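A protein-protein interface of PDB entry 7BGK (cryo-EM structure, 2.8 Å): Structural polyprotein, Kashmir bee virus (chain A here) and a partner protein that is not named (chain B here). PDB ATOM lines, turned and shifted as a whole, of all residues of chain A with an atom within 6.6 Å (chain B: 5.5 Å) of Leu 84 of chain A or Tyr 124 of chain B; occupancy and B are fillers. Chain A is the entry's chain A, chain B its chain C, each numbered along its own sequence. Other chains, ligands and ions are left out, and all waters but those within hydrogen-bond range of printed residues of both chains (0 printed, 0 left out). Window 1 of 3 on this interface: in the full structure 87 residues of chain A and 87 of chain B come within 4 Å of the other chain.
Val 59 of chain B touches Leu 39 of chain A. Gly 74 of chain A touches Val 281 of chain B. Leu 81 of chain A touches Leu 128 of chain B. Phe 83 of chain A touches Tyr 124 of chain B (CB to OH, 3.3 Å). Phe 83 of chain A touches Val 281 of chain B. OH of Tyr 85 of chain A touches CG2 of Val 59 of chain B (3.7 Å). O of Pro 197 of chain A touches CD of Pro 119 of chain B, 3.7 Å away. CD of Pro 197 of chain A touches CE1 of Tyr 124 of chain B (3.7 Å). O of Gln 198 of chain A touches CG1 of Val 281 of chain B, 3.6 Å away. Leu 199 of chain A touches Tyr 124 of chain B.
Of the 12 printed residues of chain B, 7 touch a printed residue of chain A. Hydrophobic or aromatic side chains of chain B that line the printed part of chain A: Val 59, Pro 119, Tyr 124, Leu 128 and Val 281. Among the printed residues, 21 pairs touch across the chains.
The side-chain hydroxyl (OH) of Tyr 124 of chain B sits at hydrogen-bond distance from the backbone carbonyl oxygen (O) of Tyr 80 of chain A, 2.8 Å away. The side-chain hydroxyl (OG1) of Thr 196 of chain A is in hydrogen-bond range of the backbone carbonyl oxygen (O) of Pro 119 of chain B (2.7 Å).
Of the printed residues of chain B, Gly 74 of chain A touches Val 281. Of the printed residues of chain B, Thr 196 of chain A touches Pro 119, Pro 121 and Tyr 124. Of the printed residues of chain B, Leu 39 of chain A touches Val 59. Of the printed residues of chain B, Leu 81 of chain A touches Leu 128 (3.9 Å). Of the printed residues of chain A, Pro 119 of chain B touches Thr 196, Pro 197 and Leu 199. The nearest residue of chain A that does not touch Tyr 124 of chain B is Leu 81 of chain A (4.9 Å). The nearest printed residue of chain B that does not touch Leu 81 of chain A is Tyr 124 of chain B (4.9 Å).
The backbone NH (N) of Gly 74 of chain A is in hydrogen-bond range of the side-chain hydroxyl (OG) of Ser 79 of chain A, 3.3 Å away. O of Leu 84 of chain A sits at hydrogen-bond distance from N of Ile 194 of chain A, at 2.6 Å.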
ATOM      1  N   LEU A  39     -25.586  30.476   2.745  1.00  0.00           N
ATOM      2  CA  LEU A  39     -24.455  29.568   2.654  1.00  0.00           C
ATOM      3  C   LEU A  39     -24.614  28.481   1.600  1.00  0.00           C
ATOM      4  O   LEU A  39     -23.652  27.750   1.352  1.00  0.00           O
ATOM      5  CB  LEU A  39     -24.202  28.919   4.015  1.00  0.00           C
ATOM      6  CG  LEU A  39     -24.024  29.898   5.175  1.00  0.00           C
ATOM      7  CD1 LEU A  39     -24.225  29.213   6.499  1.00  0.00           C
ATOM      8  CD2 LEU A  39     -22.670  30.546   5.136  1.00  0.00           C
ATOM      9  N   GLY A  74     -12.829  19.533   7.321  1.00  0.00           N
ATOM     10  CA  GLY A  74     -13.400  20.856   7.405  1.00  0.00           C
ATOM     11  C   GLY A  74     -12.750  21.877   6.508  1.00  0.00           C
ATOM     12  O   GLY A  74     -12.792  23.073   6.814  1.00  0.00           O
ATOM     13  N   SER A  79     -17.870  20.412   3.728  1.00  0.00           N
ATOM     14  CA  SER A  79     -17.467  19.781   4.975  1.00  0.00           C
ATOM     15  C   SER A  79     -17.529  20.726   6.162  1.00  0.00           C
ATOM     16  O   SER A  79     -18.036  20.348   7.221  1.00  0.00           O
ATOM     17  CB  SER A  79     -16.047  19.241   4.842  1.00  0.00           C
ATOM     18  OG  SER A  79     -15.653  18.546   6.005  1.00  0.00           O
ATOM     19  N   TYR A  80     -17.029  21.950   6.006  1.00  0.00           N
ATOM     20  CA  TYR A  80     -17.085  22.918   7.092  1.00  0.00           C
ATOM     21  C   TYR A  80     -18.521  23.202   7.500  1.00  0.00           C
ATOM     22  O   TYR A  80     -18.837  23.253   8.693  1.00  0.00           O
ATOM     23  CB  TYR A  80     -16.379  24.201   6.669  1.00  0.00           C
ATOM     24  CG  TYR A  80     -16.031  25.137   7.796  1.00  0.00           C
ATOM     25  CD1 TYR A  80     -14.967  24.875   8.639  1.00  0.00           C
ATOM     26  CD2 TYR A  80     -16.746  26.300   7.994  1.00  0.00           C
ATOM     27  CE1 TYR A  80     -14.645  25.735   9.656  1.00  0.00           C
ATOM     28  CE2 TYR A  80     -16.429  27.160   9.005  1.00  0.00           C
ATOM     29  CZ  TYR A  80     -15.382  26.880   9.830  1.00  0.00           C
ATOM     30  OH  TYR A  80     -15.088  27.763  10.834  1.00  0.00           O
ATOM     31  N   LEU A  81     -19.405  23.392   6.524  1.00  0.00           N
ATOM     32  CA  LEU A  81     -20.797  23.694   6.805  1.00  0.00           C
ATOM     33  C   LEU A  81     -21.606  22.466   7.189  1.00  0.00           C
ATOM     34  O   LEU A  81     -22.738  22.615   7.653  1.00  0.00           O
ATOM     35  CB  LEU A  81     -21.429  24.366   5.589  1.00  0.00           C
ATOM     36  CG  LEU A  81     -20.859  25.720   5.177  1.00  0.00           C
ATOM     37  CD1 LEU A  81     -21.495  26.188   3.898  1.00  0.00           C
ATOM     38  CD2 LEU A  81     -21.062  26.743   6.259  1.00  0.00           C
ATOM     39  N   SER A  82     -21.060  21.266   7.010  1.00  0.00           N
ATOM     40  CA  SER A  82     -21.765  20.055   7.394  1.00  0.00           C
ATOM     41  C   SER A  82     -21.731  19.809   8.893  1.00  0.00           C
ATOM     42  O   SER A  82     -22.518  19.002   9.392  1.00  0.00           O
ATOM     43  CB  SER A  82     -21.169  18.855   6.664  1.00  0.00           C
ATOM     44  OG  SER A  82     -19.859  18.585   7.112  1.00  0.00           O
ATOM     45  N   PHE A  83     -20.842  20.479   9.616  1.00  0.00           N
ATOM     46  CA  PHE A  83     -20.769  20.348  11.061  1.00  0.00           C
ATOM     47  C   PHE A  83     -21.811  21.188  11.778  1.00  0.00           C
ATOM     48  O   PHE A  83     -21.920  21.099  13.005  1.00  0.00           O
ATOM     49  CB  PHE A  83     -19.373  20.731  11.539  1.00  0.00           C
ATOM     50  CG  PHE A  83     -18.333  19.704  11.241  1.00  0.00           C
ATOM     51  CD1 PHE A  83     -18.088  18.674  12.120  1.00  0.00           C
ATOM     52  CD2 PHE A  83     -17.597  19.769  10.082  1.00  0.00           C
ATOM     53  CE1 PHE A  83     -17.135  17.735  11.844  1.00  0.00           C
ATOM     54  CE2 PHE A  83     -16.643  18.830   9.805  1.00  0.00           C
ATOM     55  CZ  PHE A  83     -16.412  17.812  10.688  1.00  0.00           C
ATOM     56  N   LEU A  84     -22.570  21.994  11.045  1.00  0.00           N
ATOM     57  CA  LEU A  84     -23.685  22.743  11.595  1.00  0.00           C
ATOM     58  C   LEU A  84     -25.019  22.040  11.414  1.00  0.00           C
ATOM     59  O   LEU A  84     -26.017  22.494  11.978  1.00  0.00           O
ATOM     60  CB  LEU A  84     -23.769  24.120  10.937  1.00  0.00           C
ATOM     61  CG  LEU A  84     -22.664  25.126  11.197  1.00  0.00           C
ATOM     62  CD1 LEU A  84     -22.792  26.247  10.210  1.00  0.00           C
ATOM     63  CD2 LEU A  84     -22.749  25.648  12.599  1.00  0.00           C
ATOM     64  N   TYR A  85     -25.060  20.954  10.648  1.00  0.00           N
ATOM     65  CA  TYR A  85     -26.306  20.316  10.266  1.00  0.00           C
ATOM     66  C   TYR A  85     -26.172  18.811  10.421  1.00  0.00           C
ATOM     67  O   TYR A  85     -25.081  18.277  10.633  1.00  0.00           O
ATOM     68  CB  TYR A  85     -26.693  20.682   8.828  1.00  0.00           C
ATOM     69  CG  TYR A  85     -26.732  22.169   8.574  1.00  0.00           C
ATOM     70  CD1 TYR A  85     -27.851  22.921   8.881  1.00  0.00           C
ATOM     71  CD2 TYR A  85     -25.643  22.823   8.038  1.00  0.00           C
ATOM     72  CE1 TYR A  85     -27.879  24.266   8.663  1.00  0.00           C
ATOM     73  CE2 TYR A  85     -25.664  24.172   7.815  1.00  0.00           C
ATOM     74  CZ  TYR A  85     -26.784  24.890   8.129  1.00  0.00           C
ATOM     75  OH  TYR A  85     -26.805  26.242   7.906  1.00  0.00           O
ATOM     76  N   ARG A  86     -27.306  18.131  10.310  1.00  0.00           N
ATOM     77  CA  ARG A  86     -27.395  16.688  10.455  1.00  0.00           C
ATOM     78  C   ARG A  86     -27.861  15.978   9.198  1.00  0.00           C
ATOM     79  O   ARG A  86     -27.469  14.833   8.974  1.00  0.00           O
ATOM     80  CB  ARG A  86     -28.353  16.325  11.597  1.00  0.00           C
ATOM     81  CG  ARG A  86     -27.836  16.613  12.980  1.00  0.00           C
ATOM     82  CD  ARG A  86     -26.533  15.909  13.257  1.00  0.00           C
ATOM     83  NE  ARG A  86     -26.357  15.615  14.671  1.00  0.00           N
ATOM     84  CZ  ARG A  86     -25.248  15.844  15.363  1.00  0.00           C
ATOM     85  NH1 ARG A  86     -24.186  16.385  14.793  1.00  0.00           N
ATOM     86  NH2 ARG A  86     -25.203  15.533  16.644  1.00  0.00           N
ATOM     87  N   GLY A 191     -29.178  20.066   6.209  1.00  0.00           N
ATOM     88  CA  GLY A 191     -30.382  19.820   6.965  1.00  0.00           C
ATOM     89  C   GLY A 191     -30.744  20.906   7.937  1.00  0.00           C
ATOM     90  O   GLY A 191     -30.861  22.072   7.556  1.00  0.00           O
ATOM     91  N   TRP A 192     -30.944  20.531   9.193  1.00  0.00           N
ATOM     92  CA  TRP A 192     -31.409  21.464  10.199  1.00  0.00           C
ATOM     93  C   TRP A 192     -30.364  21.633  11.293  1.00  0.00           C
ATOM     94  O   TRP A 192     -29.637  20.699  11.641  1.00  0.00           O
ATOM     95  CB  TRP A 192     -32.776  21.020  10.716  1.00  0.00           C
ATOM     96  CG  TRP A 192     -32.857  19.660  11.314  1.00  0.00           C
ATOM     97  CD1 TRP A 192     -33.020  18.486  10.642  1.00  0.00           C
ATOM     98  CD2 TRP A 192     -32.893  19.333  12.703  1.00  0.00           C
ATOM     99  NE1 TRP A 192     -33.117  17.445  11.526  1.00  0.00           N
ATOM    100  CE2 TRP A 192     -33.037  17.940  12.797  1.00  0.00           C
ATOM    101  CE3 TRP A 192     -32.792  20.080  13.874  1.00  0.00           C
ATOM    102  CZ2 TRP A 192     -33.085  17.283  14.004  1.00  0.00           C
ATOM    103  CZ3 TRP A 192     -32.834  19.427  15.069  1.00  0.00           C
ATOM    104  CH2 TRP A 192     -32.986  18.041  15.130  1.00  0.00           C
ATOM    105  N   MET A 193     -30.322  22.846  11.830  1.00  0.00           N
ATOM    106  CA  MET A 193     -29.113  23.398  12.412  1.00  0.00           C
ATOM    107  C   MET A 193     -28.841  22.851  13.802  1.00  0.00           C
ATOM    108  O   MET A 193     -29.755  22.570  14.582  1.00  0.00           O
ATOM    109  CB  MET A 193     -29.216  24.920  12.472  1.00  0.00           C
ATOM    110  CG  MET A 193     -27.926  25.661  12.232  1.00  0.00           C
ATOM    111  SD  MET A 193     -28.197  27.417  12.032  1.00  0.00           S
ATOM    112  CE  MET A 193     -29.028  27.779  13.565  1.00  0.00           C
ATOM    113  N   ILE A 194     -27.554  22.710  14.102  1.00  0.00           N
ATOM    114  CA  ILE A 194     -27.075  22.260  15.400  1.00  0.00           C
ATOM    115  C   ILE A 194     -25.888  23.127  15.790  1.00  0.00           C
ATOM    116  O   ILE A 194     -25.567  24.107  15.111  1.00  0.00           O
ATOM    117  CB  ILE A 194     -26.689  20.772  15.387  1.00  0.00           C
ATOM    118  CG1 ILE A 194     -25.658  20.504  14.301  1.00  0.00           C
ATOM    119  CG2 ILE A 194     -27.907  19.912  15.190  1.00  0.00           C
ATOM    120  CD1 ILE A 194     -24.968  19.236  14.453  1.00  0.00           C
ATOM    121  N   GLY A 195     -25.239  22.775  16.883  1.00  0.00           N
ATOM    122  CA  GLY A 195     -24.114  23.535  17.371  1.00  0.00           C
ATOM    123  C   GLY A 195     -22.831  23.259  16.628  1.00  0.00           C
ATOM    124  O   GLY A 195     -22.706  22.313  15.853  1.00  0.00           O
ATOM    125  N   THR A 196     -21.879  24.102  16.877  1.00  0.00           N
ATOM    126  CA  THR A 196     -20.568  24.060  16.257  1.00  0.00           C
ATOM    127  C   THR A 196     -19.631  23.113  16.997  1.00  0.00           C
ATOM    128  O   THR A 196     -19.812  22.855  18.190  1.00  0.00           O
ATOM    129  CB  THR A 196     -19.958  25.454  16.249  1.00  0.00           C
ATOM    130  OG1 THR A 196     -19.884  25.947  17.590  1.00  0.00           O
ATOM    131  CG2 THR A 196     -20.791  26.379  15.443  1.00  0.00           C
ATOM    132  N   PRO A 197     -18.629  22.573  16.303  1.00  0.00           N
ATOM    133  CA  PRO A 197     -17.533  21.887  16.992  1.00  0.00           C
ATOM    134  C   PRO A 197     -16.382  22.823  17.322  1.00  0.00           C
ATOM    135  O   PRO A 197     -16.459  24.022  17.043  1.00  0.00           O
ATOM    136  CB  PRO A 197     -17.123  20.816  15.980  1.00  0.00           C
ATOM    137  CG  PRO A 197     -17.406  21.432  14.673  1.00  0.00           C
ATOM    138  CD  PRO A 197     -18.528  22.409  14.844  1.00  0.00           C
ATOM    139  N   GLN A 198     -15.314  22.297  17.919  1.00  0.00           N
ATOM    140  CA  GLN A 198     -14.115  23.096  18.092  1.00  0.00           C
ATOM    141  C   GLN A 198     -13.408  23.264  16.751  1.00  0.00           C
ATOM    142  O   GLN A 198     -13.644  22.520  15.797  1.00  0.00           O
ATOM    143  CB  GLN A 198     -13.148  22.464  19.096  1.00  0.00           C
ATOM    144  CG  GLN A 198     -13.554  22.505  20.563  1.00  0.00           C
ATOM    145  CD  GLN A 198     -14.621  21.516  20.901  1.00  0.00           C
ATOM    146  OE1 GLN A 198     -15.713  21.878  21.328  1.00  0.00           O
ATOM    147  NE2 GLN A 198     -14.298  20.244  20.742  1.00  0.00           N
ATOM    148  N   LEU A 199     -12.540  24.265  16.682  1.00  0.00           N
ATOM    149  CA  LEU A 199     -11.710  24.503  15.514  1.00  0.00           C
ATOM    150  C   LEU A 199     -10.246  24.276  15.865  1.00  0.00           C
ATOM    151  O   LEU A 199      -9.817  24.506  16.997  1.00  0.00           O
ATOM    152  CB  LEU A 199     -11.898  25.917  14.967  1.00  0.00           C
ATOM    153  CG  LEU A 199     -13.239  26.218  14.307  1.00  0.00           C
ATOM    154  CD1 LEU A 199     -13.345  27.686  13.998  1.00  0.00           C
ATOM    155  CD2 LEU A 199     -13.433  25.414  13.047  1.00  0.00           C
ATOM    156  N   VAL B  59     -27.951  31.360  11.121  1.00  0.00           N
ATOM    157  CA  VAL B  59     -26.809  30.735  11.775  1.00  0.00           C
ATOM    158  C   VAL B  59     -26.195  31.683  12.793  1.00  0.00           C
ATOM    159  O   VAL B  59     -26.048  31.347  13.973  1.00  0.00           O
ATOM    160  CB  VAL B  59     -25.770  30.291  10.732  1.00  0.00           C
ATOM    161  CG1 VAL B  59     -24.718  29.428  11.370  1.00  0.00           C
ATOM    162  CG2 VAL B  59     -26.425  29.552   9.599  1.00  0.00           C
ATOM    163  N   PRO B 119     -15.731  28.268  19.075  1.00  0.00           N
ATOM    164  CA  PRO B 119     -16.594  29.108  18.246  1.00  0.00           C
ATOM    165  C   PRO B 119     -18.065  28.989  18.599  1.00  0.00           C
ATOM    166  O   PRO B 119     -18.575  27.906  18.893  1.00  0.00           O
ATOM    167  CB  PRO B 119     -16.344  28.575  16.831  1.00  0.00           C
ATOM    168  CG  PRO B 119     -15.119  27.830  16.907  1.00  0.00           C
ATOM    169  CD  PRO B 119     -15.113  27.217  18.258  1.00  0.00           C
ATOM    170  N   ALA B 120     -18.742  30.120  18.561  1.00  0.00           N
ATOM    171  CA  ALA B 120     -20.190  30.157  18.483  1.00  0.00           C
ATOM    172  C   ALA B 120     -20.609  30.142  17.025  1.00  0.00           C
ATOM    173  O   ALA B 120     -19.795  30.350  16.125  1.00  0.00           O
ATOM    174  CB  ALA B 120     -20.718  31.394  19.201  1.00  0.00           C
ATOM    175  N   PRO B 121     -21.883  29.883  16.741  1.00  0.00           N
ATOM    176  CA  PRO B 121     -22.307  29.805  15.337  1.00  0.00           C
ATOM    177  C   PRO B 121     -22.000  31.057  14.536  1.00  0.00           C
ATOM    178  O   PRO B 121     -21.883  30.975  13.309  1.00  0.00           O
ATOM    179  CB  PRO B 121     -23.813  29.555  15.448  1.00  0.00           C
ATOM    180  CG  PRO B 121     -23.981  28.927  16.776  1.00  0.00           C
ATOM    181  CD  PRO B 121     -22.983  29.555  17.660  1.00  0.00           C
ATOM    182  N   CYS B 122     -21.873  32.211  15.188  1.00  0.00           N
ATOM    183  CA  CYS B 122     -21.461  33.427  14.502  1.00  0.00           C
ATOM    184  C   CYS B 122     -19.970  33.438  14.207  1.00  0.00           C
ATOM    185  O   CYS B 122     -19.544  34.008  13.197  1.00  0.00           O
ATOM    186  CB  CYS B 122     -21.824  34.643  15.350  1.00  0.00           C
ATOM    187  SG  CYS B 122     -20.967  34.729  16.917  1.00  0.00           S
ATOM    188  N   GLU B 123     -19.172  32.816  15.072  1.00  0.00           N
ATOM    189  CA  GLU B 123     -17.730  32.754  14.898  1.00  0.00           C
ATOM    190  C   GLU B 123     -17.310  31.647  13.946  1.00  0.00           C
ATOM    191  O   GLU B 123     -16.222  31.722  13.367  1.00  0.00           O
ATOM    192  CB  GLU B 123     -17.064  32.553  16.257  1.00  0.00           C
ATOM    193  CG  GLU B 123     -17.799  33.221  17.397  1.00  0.00           C
ATOM    194  CD  GLU B 123     -16.985  33.318  18.661  1.00  0.00           C
ATOM    195  OE1 GLU B 123     -16.238  32.369  18.962  1.00  0.00           O
ATOM    196  OE2 GLU B 123     -17.096  34.343  19.361  1.00  0.00           O
ATOM    197  N   TYR B 124     -18.147  30.623  13.783  1.00  0.00           N
ATOM    198  CA  TYR B 124     -17.887  29.575  12.807  1.00  0.00           C
ATOM    199  C   TYR B 124     -18.016  30.109  11.388  1.00  0.00           C
ATOM    200  O   TYR B 124     -17.251  29.724  10.498  1.00  0.00           O
ATOM    201  CB  TYR B 124     -18.866  28.430  13.051  1.00  0.00           C
ATOM    202  CG  TYR B 124     -18.457  27.074  12.533  1.00  0.00           C
ATOM    203  CD1 TYR B 124     -17.448  26.353  13.144  1.00  0.00           C
ATOM    204  CD2 TYR B 124     -19.116  26.494  11.466  1.00  0.00           C
ATOM    205  CE1 TYR B 124     -17.088  25.114  12.687  1.00  0.00           C
ATOM    206  CE2 TYR B 124     -18.763  25.255  11.005  1.00  0.00           C
ATOM    207  CZ  TYR B 124     -17.752  24.569  11.617  1.00  0.00           C
ATOM    208  OH  TYR B 124     -17.410  23.328  11.141  1.00  0.00           O
ATOM    209  N   VAL B 125     -18.977  31.004  11.165  1.00  0.00           N
ATOM    210  CA  VAL B 125     -19.220  31.552   9.838  1.00  0.00           C
ATOM    211  C   VAL B 125     -18.152  32.572   9.472  1.00  0.00           C
ATOM    212  O   VAL B 125     -17.605  32.551   8.364  1.00  0.00           O
ATOM    213  CB  VAL B 125     -20.633  32.166   9.789  1.00  0.00           C
ATOM    214  CG1 VAL B 125     -20.837  33.022   8.548  1.00  0.00           C
ATOM    215  CG2 VAL B 125     -21.679  31.079   9.873  1.00  0.00           C
ATOM    216  N   ALA B 126     -17.848  33.484  10.393  1.00  0.00           N
ATOM    217  CA  ALA B 126     -16.840  34.503  10.133  1.00  0.00           C
ATOM    218  C   ALA B 126     -15.505  33.896   9.732  1.00  0.00           C
ATOM    219  O   ALA B 126     -14.769  34.490   8.937  1.00  0.00           O
ATOM    220  CB  ALA B 126     -16.670  35.385  11.366  1.00  0.00           C
ATOM    221  N   ASN B 127     -15.170  32.726  10.267  1.00  0.00           N
ATOM    222  CA  ASN B 127     -13.886  32.109   9.968  1.00  0.00           C
ATOM    223  C   ASN B 127     -13.766  31.701   8.507  1.00  0.00           C
ATOM    224  O   ASN B 127     -12.648  31.495   8.025  1.00  0.00           O
ATOM    225  CB  ASN B 127     -13.677  30.892  10.867  1.00  0.00           C
ATOM    226  CG  ASN B 127     -12.223  30.577  11.090  1.00  0.00           C
ATOM    227  OD1 ASN B 127     -11.467  31.396  11.610  1.00  0.00           O
ATOM    228  ND2 ASN B 127     -11.816  29.384  10.694  1.00  0.00           N
ATOM    229  N   LEU B 128     -14.882  31.586   7.797  1.00  0.00           N
ATOM    230  CA  LEU B 128     -14.869  31.240   6.385  1.00  0.00           C
ATOM    231  C   LEU B 128     -14.571  32.427   5.487  1.00  0.00           C
ATOM    232  O   LEU B 128     -14.412  32.242   4.278  1.00  0.00           O
ATOM    233  CB  LEU B 128     -16.213  30.650   5.972  1.00  0.00           C
ATOM    234  CG  LEU B 128     -16.460  29.170   6.197  1.00  0.00           C
ATOM    235  CD1 LEU B 128     -17.868  28.858   5.773  1.00  0.00           C
ATOM    236  CD2 LEU B 128     -15.465  28.301   5.461  1.00  0.00           C
ATOM    237  N   VAL B 281     -11.526  21.598  11.322  1.00  0.00           N
ATOM    238  CA  VAL B 281     -12.322  21.231  12.483  1.00  0.00           C
ATOM    239  C   VAL B 281     -11.490  20.331  13.380  1.00  0.00           C
ATOM    240  O   VAL B 281     -10.800  19.422  12.909  1.00  0.00           O
ATOM    241  CB  VAL B 281     -13.631  20.540  12.055  1.00  0.00           C
ATOM    242  CG1 VAL B 281     -14.461  20.169  13.257  1.00  0.00           C
ATOM    243  CG2 VAL B 281     -14.422  21.441  11.146  1.00  0.00           C
